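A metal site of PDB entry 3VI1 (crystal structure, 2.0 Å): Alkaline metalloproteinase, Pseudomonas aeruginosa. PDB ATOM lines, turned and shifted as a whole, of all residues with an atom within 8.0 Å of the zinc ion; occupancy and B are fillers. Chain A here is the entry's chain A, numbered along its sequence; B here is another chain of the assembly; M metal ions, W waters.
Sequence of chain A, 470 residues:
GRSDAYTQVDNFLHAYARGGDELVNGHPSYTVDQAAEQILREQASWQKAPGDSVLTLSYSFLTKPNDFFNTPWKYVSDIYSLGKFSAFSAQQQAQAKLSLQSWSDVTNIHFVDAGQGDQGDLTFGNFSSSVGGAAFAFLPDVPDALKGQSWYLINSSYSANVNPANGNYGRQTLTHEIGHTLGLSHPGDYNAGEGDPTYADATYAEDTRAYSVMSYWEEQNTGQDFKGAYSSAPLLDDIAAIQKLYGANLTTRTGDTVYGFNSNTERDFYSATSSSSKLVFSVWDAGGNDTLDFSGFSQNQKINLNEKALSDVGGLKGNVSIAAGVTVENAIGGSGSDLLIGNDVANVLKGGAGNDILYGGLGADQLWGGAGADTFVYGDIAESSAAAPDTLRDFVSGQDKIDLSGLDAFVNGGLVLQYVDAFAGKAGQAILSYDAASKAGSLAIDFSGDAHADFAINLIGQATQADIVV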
ATOM      1  N   ALA A 135       1.154 -16.021  -7.701  1.00  0.00           N
ATOM      2  CA  ALA A 135       2.026 -15.786  -8.847  1.00  0.00           C
ATOM      3  C   ALA A 135       1.904 -16.978  -9.796  1.00  0.00           C
ATOM      4  O   ALA A 135       1.455 -18.039  -9.391  1.00  0.00           O
ATOM      5  CB  ALA A 135       3.473 -15.627  -8.401  1.00  0.00           C
ATOM      6  N   PHE A 136       2.296 -16.786 -11.051  1.00  0.00           N
ATOM      7  CA  PHE A 136       2.317 -17.887 -12.015  1.00  0.00           C
ATOM      8  C   PHE A 136       3.411 -17.750 -13.078  1.00  0.00           C
ATOM      9  O   PHE A 136       3.863 -16.640 -13.375  1.00  0.00           O
ATOM     10  CB  PHE A 136       0.942 -18.119 -12.661  1.00  0.00           C
ATOM     11  CG  PHE A 136       0.458 -16.975 -13.524  1.00  0.00           C
ATOM     12  CD1 PHE A 136       0.780 -16.931 -14.879  1.00  0.00           C
ATOM     13  CD2 PHE A 136      -0.341 -15.966 -12.991  1.00  0.00           C
ATOM     14  CE1 PHE A 136       0.322 -15.880 -15.686  1.00  0.00           C
ATOM     15  CE2 PHE A 136      -0.795 -14.920 -13.791  1.00  0.00           C
ATOM     16  CZ  PHE A 136      -0.460 -14.881 -15.143  1.00  0.00           C
ATOM     17  N   ALA A 137       3.846 -18.884 -13.624  1.00  0.00           N
ATOM     18  CA  ALA A 137       4.845 -18.915 -14.684  1.00  0.00           C
ATOM     19  C   ALA A 137       4.565 -20.038 -15.677  1.00  0.00           C
ATOM     20  O   ALA A 137       3.776 -20.948 -15.390  1.00  0.00           O
ATOM     21  CB  ALA A 137       6.250 -19.055 -14.101  1.00  0.00           C
ATOM     22  N   LEU A 139       6.165 -23.137 -18.084  1.00  0.00           N
ATOM     23  CA  LEU A 139       7.262 -24.062 -18.363  1.00  0.00           C
ATOM     24  C   LEU A 139       7.710 -23.909 -19.828  1.00  0.00           C
ATOM     25  O   LEU A 139       6.895 -23.561 -20.679  1.00  0.00           O
ATOM     26  CB  LEU A 139       6.842 -25.506 -18.067  1.00  0.00           C
ATOM     27  CG  LEU A 139       6.928 -25.999 -16.616  1.00  0.00           C
ATOM     28  CD1 LEU A 139       5.789 -25.458 -15.749  1.00  0.00           C
ATOM     29  CD2 LEU A 139       6.917 -27.515 -16.588  1.00  0.00           C
ATOM     30  N   THR A 173       9.073 -17.053  -3.755  1.00  0.00           N
ATOM     31  CA  THR A 173       8.149 -17.028  -4.892  1.00  0.00           C
ATOM     32  C   THR A 173       8.902 -16.756  -6.200  1.00  0.00           C
ATOM     33  O   THR A 173       8.657 -17.432  -7.205  1.00  0.00           O
ATOM     34  CB  THR A 173       7.021 -15.991  -4.680  1.00  0.00           C
ATOM     35  OG1 THR A 173       6.377 -16.221  -3.426  1.00  0.00           O
ATOM     36  CG2 THR A 173       5.990 -16.081  -5.798  1.00  0.00           C
ATOM     37  N   HIS A 176      10.913 -19.729  -6.995  1.00  0.00           N
ATOM     38  CA  HIS A 176       9.920 -20.740  -7.358  1.00  0.00           C
ATOM     39  C   HIS A 176       9.438 -20.568  -8.805  1.00  0.00           C
ATOM     40  O   HIS A 176       9.440 -21.537  -9.581  1.00  0.00           O
ATOM     41  CB  HIS A 176       8.748 -20.677  -6.371  1.00  0.00           C
ATOM     42  CG  HIS A 176       7.579 -21.529  -6.735  1.00  0.00           C
ATOM     43  ND1 HIS A 176       7.346 -22.758  -6.147  1.00  0.00           N
ATOM     44  CD2 HIS A 176       6.545 -21.325  -7.582  1.00  0.00           C
ATOM     45  CE1 HIS A 176       6.239 -23.281  -6.652  1.00  0.00           C
ATOM     46  NE2 HIS A 176       5.729 -22.426  -7.522  1.00  0.00           N
ATOM     47  N   GLU A 177       9.050 -19.350  -9.175  1.00  0.00           N
ATOM     48  CA  GLU A 177       8.521 -19.058 -10.507  1.00  0.00           C
ATOM     49  C   GLU A 177       9.572 -19.190 -11.608  1.00  0.00           C
ATOM     50  O   GLU A 177       9.272 -19.661 -12.710  1.00  0.00           O
ATOM     51  CB  GLU A 177       7.867 -17.676 -10.557  1.00  0.00           C
ATOM     52  CG  GLU A 177       6.665 -17.479  -9.636  1.00  0.00           C
ATOM     53  CD  GLU A 177       5.527 -18.463  -9.869  1.00  0.00           C
ATOM     54  OE1 GLU A 177       5.350 -18.927 -11.016  1.00  0.00           O
ATOM     55  OE2 GLU A 177       4.803 -18.768  -8.908  1.00  0.00           O
ATOM     56  N   GLY A 179      12.120 -21.188 -11.364  1.00  0.00           N
ATOM     57  CA  GLY A 179      12.193 -22.643 -11.417  1.00  0.00           C
ATOM     58  C   GLY A 179      11.243 -23.239 -12.452  1.00  0.00           C
ATOM     59  O   GLY A 179      11.625 -24.129 -13.201  1.00  0.00           O
ATOM     60  N   HIS A 180      10.011 -22.733 -12.482  1.00  0.00           N
ATOM     61  CA  HIS A 180       9.044 -23.136 -13.499  1.00  0.00           C
ATOM     62  C   HIS A 180       9.513 -22.816 -14.917  1.00  0.00           C
ATOM     63  O   HIS A 180       9.488 -23.681 -15.793  1.00  0.00           O
ATOM     64  CB  HIS A 180       7.675 -22.488 -13.263  1.00  0.00           C
ATOM     65  CG  HIS A 180       6.873 -23.125 -12.168  1.00  0.00           C
ATOM     66  ND1 HIS A 180       6.555 -24.469 -12.157  1.00  0.00           N
ATOM     67  CD2 HIS A 180       6.294 -22.596 -11.061  1.00  0.00           C
ATOM     68  CE1 HIS A 180       5.835 -24.738 -11.084  1.00  0.00           C
ATOM     69  NE2 HIS A 180       5.661 -23.620 -10.409  1.00  0.00           N
ATOM     70  N   LEU A 184      10.991 -26.715 -14.177  1.00  0.00           N
ATOM     71  CA  LEU A 184      10.590 -27.465 -12.983  1.00  0.00           C
ATOM     72  C   LEU A 184       9.094 -27.314 -12.695  1.00  0.00           C
ATOM     73  O   LEU A 184       8.507 -26.251 -12.937  1.00  0.00           O
ATOM     74  CB  LEU A 184      11.398 -27.025 -11.757  1.00  0.00           C
ATOM     75  CG  LEU A 184      12.929 -26.923 -11.807  1.00  0.00           C
ATOM     76  CD1 LEU A 184      13.457 -26.643 -10.413  1.00  0.00           C
ATOM     77  CD2 LEU A 184      13.583 -28.168 -12.381  1.00  0.00           C
ATOM     78  N   SER A 185       8.500 -28.388 -12.199  1.00  0.00           N
ATOM     79  CA  SER A 185       7.093 -28.378 -11.776  1.00  0.00           C
ATOM     80  C   SER A 185       7.027 -28.502 -10.253  1.00  0.00           C
ATOM     81  O   SER A 185       8.035 -28.764  -9.600  1.00  0.00           O
ATOM     82  CB  SER A 185       6.339 -29.539 -12.423  1.00  0.00           C
ATOM     83  OG  SER A 185       6.243 -29.379 -13.827  1.00  0.00           O
ATOM     84  N   HIS A 186       5.831 -28.295  -9.705  1.00  0.00           N
ATOM     85  CA  HIS A 186       5.550 -28.670  -8.314  1.00  0.00           C
ATOM     86  C   HIS A 186       5.783 -30.168  -8.191  1.00  0.00           C
ATOM     87  O   HIS A 186       5.418 -30.926  -9.097  1.00  0.00           O
ATOM     88  CB  HIS A 186       4.104 -28.342  -7.923  1.00  0.00           C
ATOM     89  CG  HIS A 186       3.704 -26.922  -8.182  1.00  0.00           C
ATOM     90  ND1 HIS A 186       2.445 -26.581  -8.630  1.00  0.00           N
ATOM     91  CD2 HIS A 186       4.396 -25.762  -8.075  1.00  0.00           C
ATOM     92  CE1 HIS A 186       2.373 -25.271  -8.777  1.00  0.00           C
ATOM     93  NE2 HIS A 186       3.544 -24.750  -8.448  1.00  0.00           N
ATOM     94  N   PRO A 187       6.413 -30.609  -7.086  1.00  0.00           N
ATOM     95  CA  PRO A 187       6.733 -32.031  -6.891  1.00  0.00           C
ATOM     96  C   PRO A 187       5.510 -32.958  -6.862  1.00  0.00           C
ATOM     97  O   PRO A 187       5.670 -34.174  -6.750  1.00  0.00           O
ATOM     98  CB  PRO A 187       7.460 -32.053  -5.549  1.00  0.00           C
ATOM     99  CG  PRO A 187       7.981 -30.665  -5.375  1.00  0.00           C
ATOM    100  CD  PRO A 187       6.927 -29.793  -5.970  1.00  0.00           C
ATOM    101  N   TYR A 190      -0.670 -30.846  -8.182  1.00  0.00           N
ATOM    102  CA  TYR A 190      -1.561 -29.885  -7.543  1.00  0.00           C
ATOM    103  C   TYR A 190      -1.310 -28.472  -8.047  1.00  0.00           C
ATOM    104  O   TYR A 190      -0.201 -28.144  -8.500  1.00  0.00           O
ATOM    105  CB  TYR A 190      -1.441 -29.939  -6.018  1.00  0.00           C
ATOM    106  CG  TYR A 190      -0.029 -29.885  -5.480  1.00  0.00           C
ATOM    107  CD1 TYR A 190       0.618 -31.035  -5.054  1.00  0.00           C
ATOM    108  CD2 TYR A 190       0.660 -28.674  -5.404  1.00  0.00           C
ATOM    109  CE1 TYR A 190       1.919 -30.986  -4.554  1.00  0.00           C
ATOM    110  CE2 TYR A 190       1.966 -28.620  -4.916  1.00  0.00           C
ATOM    111  CZ  TYR A 190       2.578 -29.782  -4.492  1.00  0.00           C
ATOM    112  OH  TYR A 190       3.872 -29.736  -4.004  1.00  0.00           O
ATOM    113  N   ASN A 191      -2.337 -27.628  -7.973  1.00  0.00           N
ATOM    114  CA  ASN A 191      -2.266 -26.267  -8.471  1.00  0.00           C
ATOM    115  C   ASN A 191      -3.211 -25.348  -7.715  1.00  0.00           C
ATOM    116  O   ASN A 191      -4.361 -25.701  -7.464  1.00  0.00           O
ATOM    117  CB  ASN A 191      -2.588 -26.246  -9.967  1.00  0.00           C
ATOM    118  CG  ASN A 191      -2.006 -25.046 -10.687  1.00  0.00           C
ATOM    119  OD1 ASN A 191      -2.705 -24.372 -11.450  1.00  0.00           O
ATOM    120  ND2 ASN A 191      -0.733 -24.779 -10.446  1.00  0.00           N
ATOM    121  N   ALA A 192      -2.715 -24.169  -7.340  1.00  0.00           N
ATOM    122  CA  ALA A 192      -3.515 -23.162  -6.640  1.00  0.00           C
ATOM    123  C   ALA A 192      -4.640 -22.641  -7.532  1.00  0.00           C
ATOM    124  O   ALA A 192      -4.399 -22.246  -8.682  1.00  0.00           O
ATOM    125  CB  ALA A 192      -2.639 -22.020  -6.145  1.00  0.00           C
ATOM    126  N   ARG A 209       8.676 -27.795   1.856  1.00  0.00           N
ATOM    127  CA  ARG A 209       9.546 -26.643   1.659  1.00  0.00           C
ATOM    128  C   ARG A 209      10.867 -26.753   2.421  1.00  0.00           C
ATOM    129  O   ARG A 209      11.591 -25.767   2.580  1.00  0.00           O
ATOM    130  CB  ARG A 209       8.808 -25.342   1.988  1.00  0.00           C
ATOM    131  CG  ARG A 209       7.945 -24.871   0.826  1.00  0.00           C
ATOM    132  CD  ARG A 209       6.928 -23.821   1.223  1.00  0.00           C
ATOM    133  NE  ARG A 209       6.204 -23.349   0.044  1.00  0.00           N
ATOM    134  CZ  ARG A 209       5.132 -22.568   0.060  1.00  0.00           C
ATOM    135  NH1 ARG A 209       4.630 -22.144   1.215  1.00  0.00           N
ATOM    136  NH2 ARG A 209       4.561 -22.210  -1.077  1.00  0.00           N
ATOM    137  N   VAL A 213      11.812 -25.714  -3.130  1.00  0.00           N
ATOM    138  CA  VAL A 213      11.085 -24.434  -3.184  1.00  0.00           C
ATOM    139  C   VAL A 213       9.868 -24.525  -4.118  1.00  0.00           C
ATOM    140  O   VAL A 213       9.017 -23.640  -4.120  1.00  0.00           O
ATOM    141  CB  VAL A 213      11.999 -23.245  -3.599  1.00  0.00           C
ATOM    142  CG1 VAL A 213      13.123 -23.034  -2.593  1.00  0.00           C
ATOM    143  CG2 VAL A 213      12.559 -23.437  -5.022  1.00  0.00           C
ATOM    144  N   MET A 214       9.813 -25.598  -4.907  1.00  0.00           N
ATOM    145  CA  MET A 214       8.685 -25.857  -5.813  1.00  0.00           C
ATOM    146  C   MET A 214       7.481 -26.424  -5.052  1.00  0.00           C
ATOM    147  O   MET A 214       6.375 -26.479  -5.590  1.00  0.00           O
ATOM    148  CB  MET A 214       9.102 -26.814  -6.936  1.00  0.00           C
ATOM    149  CG  MET A 214      10.344 -26.396  -7.722  1.00  0.00           C
ATOM    150  SD  MET A 214      10.260 -24.735  -8.425  1.00  0.00           S
ATOM    151  CE  MET A 214       8.967 -24.927  -9.645  1.00  0.00           C
ATOM    152  N   SER A 215       7.720 -26.838  -3.809  1.00  0.00           N
ATOM    153  CA  SER A 215       6.659 -27.395  -2.971  1.00  0.00           C
ATOM    154  C   SER A 215       5.745 -26.322  -2.403  1.00  0.00           C
ATOM    155  O   SER A 215       6.153 -25.175  -2.212  1.00  0.00           O
ATOM    156  CB  SER A 215       7.274 -28.200  -1.824  1.00  0.00           C
ATOM    157  OG  SER A 215       6.267 -28.833  -1.050  1.00  0.00           O
ATOM    158  N   TYR A 216       4.495 -26.705  -2.147  1.00  0.00           N
ATOM    159  CA  TYR A 216       3.507 -25.841  -1.510  1.00  0.00           C
ATOM    160  C   TYR A 216       3.519 -26.024   0.013  1.00  0.00           C
ATOM    161  O   TYR A 216       3.085 -25.135   0.749  1.00  0.00           O
ATOM    162  CB  TYR A 216       2.110 -26.216  -2.018  1.00  0.00           C
ATOM    163  CG  TYR A 216       1.626 -25.513  -3.273  1.00  0.00           C
ATOM    164  CD1 TYR A 216       2.512 -24.947  -4.185  1.00  0.00           C
ATOM    165  CD2 TYR A 216       0.262 -25.464  -3.560  1.00  0.00           C
ATOM    166  CE1 TYR A 216       2.059 -24.318  -5.334  1.00  0.00           C
ATOM    167  CE2 TYR A 216      -0.212 -24.843  -4.705  1.00  0.00           C
ATOM    168  CZ  TYR A 216       0.687 -24.270  -5.592  1.00  0.00           C
ATOM    169  OH  TYR A 216       0.221 -23.658  -6.721  1.00  0.00           O
ATOM    170  N   PRO B   2      -1.027 -22.141 -17.076  1.00  0.00           N
ATOM    171  CA  PRO B   2       0.208 -21.882 -16.353  1.00  0.00           C
ATOM    172  C   PRO B   2       0.324 -22.728 -15.096  1.00  0.00           C
ATOM    173  O   PRO B   2      -0.238 -23.818 -15.028  1.00  0.00           O
ATOM    174  CB  PRO B   2       0.060 -20.404 -15.975  1.00  0.00           C
ATOM    175  CG  PRO B   2      -1.430 -20.198 -15.849  1.00  0.00           C
ATOM    176  CD  PRO B   2      -2.136 -21.333 -16.556  1.00  0.00           C
ATOM    177  N   LYS B   3       1.055 -22.229 -14.103  1.00  0.00           N
ATOM    178  CA  LYS B   3       1.247 -22.951 -12.841  1.00  0.00           C
ATOM    179  C   LYS B   3       1.398 -22.003 -11.651  1.00  0.00           C
ATOM    180  O   LYS B   3       2.506 -21.669 -11.256  1.00  0.00           O
ATOM    181  CB  LYS B   3       2.453 -23.885 -12.935  1.00  0.00           C
ATOM    182  CG  LYS B   3       2.213 -25.138 -13.761  1.00  0.00           C
ATOM    183  CD  LYS B   3       1.127 -26.007 -13.140  1.00  0.00           C
ATOM    184  CE  LYS B   3       0.849 -27.234 -13.995  1.00  0.00           C
ATOM    185  NZ  LYS B   3       0.367 -26.864 -15.351  1.00  0.00           N
ATOM    186  N   PRO B   4       0.263 -21.567 -11.088  1.00  0.00           N
ATOM    187  CA  PRO B   4       0.153 -20.706  -9.912  1.00  0.00           C
ATOM    188  C   PRO B   4       0.992 -21.128  -8.693  1.00  0.00           C
ATOM    189  O   PRO B   4       1.543 -22.225  -8.664  1.00  0.00           O
ATOM    190  CB  PRO B   4      -1.334 -20.782  -9.569  1.00  0.00           C
ATOM    191  CG  PRO B   4      -1.999 -20.954 -10.888  1.00  0.00           C
ATOM    192  CD  PRO B   4      -1.028 -21.699 -11.777  1.00  0.00           C
ATOM    193  N   GLN B   5       1.064 -20.239  -7.709  1.00  0.00           N
ATOM    194  CA  GLN B   5       1.789 -20.468  -6.461  1.00  0.00           C
ATOM    195  C   GLN B   5       0.862 -20.203  -5.285  1.00  0.00           C
ATOM    196  O   GLN B   5       0.027 -19.294  -5.344  1.00  0.00           O
ATOM    197  CB  GLN B   5       3.016 -19.554  -6.397  1.00  0.00           C
ATOM    198  CG  GLN B   5       3.576 -19.293  -5.006  1.00  0.00           C
ATOM    199  CD  GLN B   5       4.460 -20.416  -4.501  1.00  0.00           C
ATOM    200  OE1 GLN B   5       5.517 -20.172  -3.919  1.00  0.00           O
ATOM    201  NE2 GLN B   5       4.041 -21.646  -4.728  1.00  0.00           N
ATOM    202  N   GLN B   6       0.995 -20.985  -4.214  1.00  0.00           N
ATOM    203  CA  GLN B   6       0.149 -20.856  -3.025  1.00  0.00           C
ATOM    204  C   GLN B   6       0.333 -19.519  -2.311  1.00  0.00           C
ATOM    205  O   GLN B   6       1.399 -18.908  -2.377  1.00  0.00           O
ATOM    206  CB  GLN B   6       0.407 -22.009  -2.053  1.00  0.00           C
ATOM    207  CG  GLN B   6      -0.534 -22.036  -0.840  1.00  0.00           C
ATOM    208  CD  GLN B   6      -0.373 -23.278   0.020  1.00  0.00           C
ATOM    209  OE1 GLN B   6      -0.279 -24.398  -0.486  1.00  0.00           O
ATOM    210  NE2 GLN B   6      -0.335 -23.086   1.332  1.00  0.00           N
HETATM  211 ZN    ZN M   1       4.278 -22.866  -8.889  1.00  0.00          ZN
HETATM  212  O   HOH W   1       4.053 -21.086  -9.443  1.00  0.00           O
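NE2 of Gln 5 of chain B sits close to NE2 of His 176 (3.4 Å). ND1 of His 176 lies within hydrogen-bond range of O of Val 213, 2.8 Å away. O of Pro 4 of chain B sits close to NE2 of His 186 (3.2 Å). A ring nitrogen (ND1) of His 186 is in hydrogen-bond range of the backbone carbonyl oxygen of Tyr 190 (3.1 Å). ND1 of His 180 lies within hydrogen-bond range of O of Leu 184 (2.8 Å). The side-chain hydroxyl (OH) of Tyr 216 lies within hydrogen-bond range of the backbone carbonyl oxygen (O) of Pro 4 of chain B (2.8 Å). The backbone carbonyl oxygen (O) of Ala 137 sits at hydrogen-bond distance from the backbone NH (N) of Lys 3 of chain B, 3.3 Å away.
Lys 3 of chain B touches the zinc ion (O to ZN, 3.2 Å). The nearest printed residue that does not touch the zinc ion is Glu 177 (4.1 Å).
The zinc ion is bound by water W1 (1.9 Å), NE2 of His 176 (2.0 Å), NE2 of His 186 (2.1 Å) and NE2 of His 180 (2.2 Å). Slightly farther from the zinc ion lies O of Pro 4 of chain B (2.8 Å).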
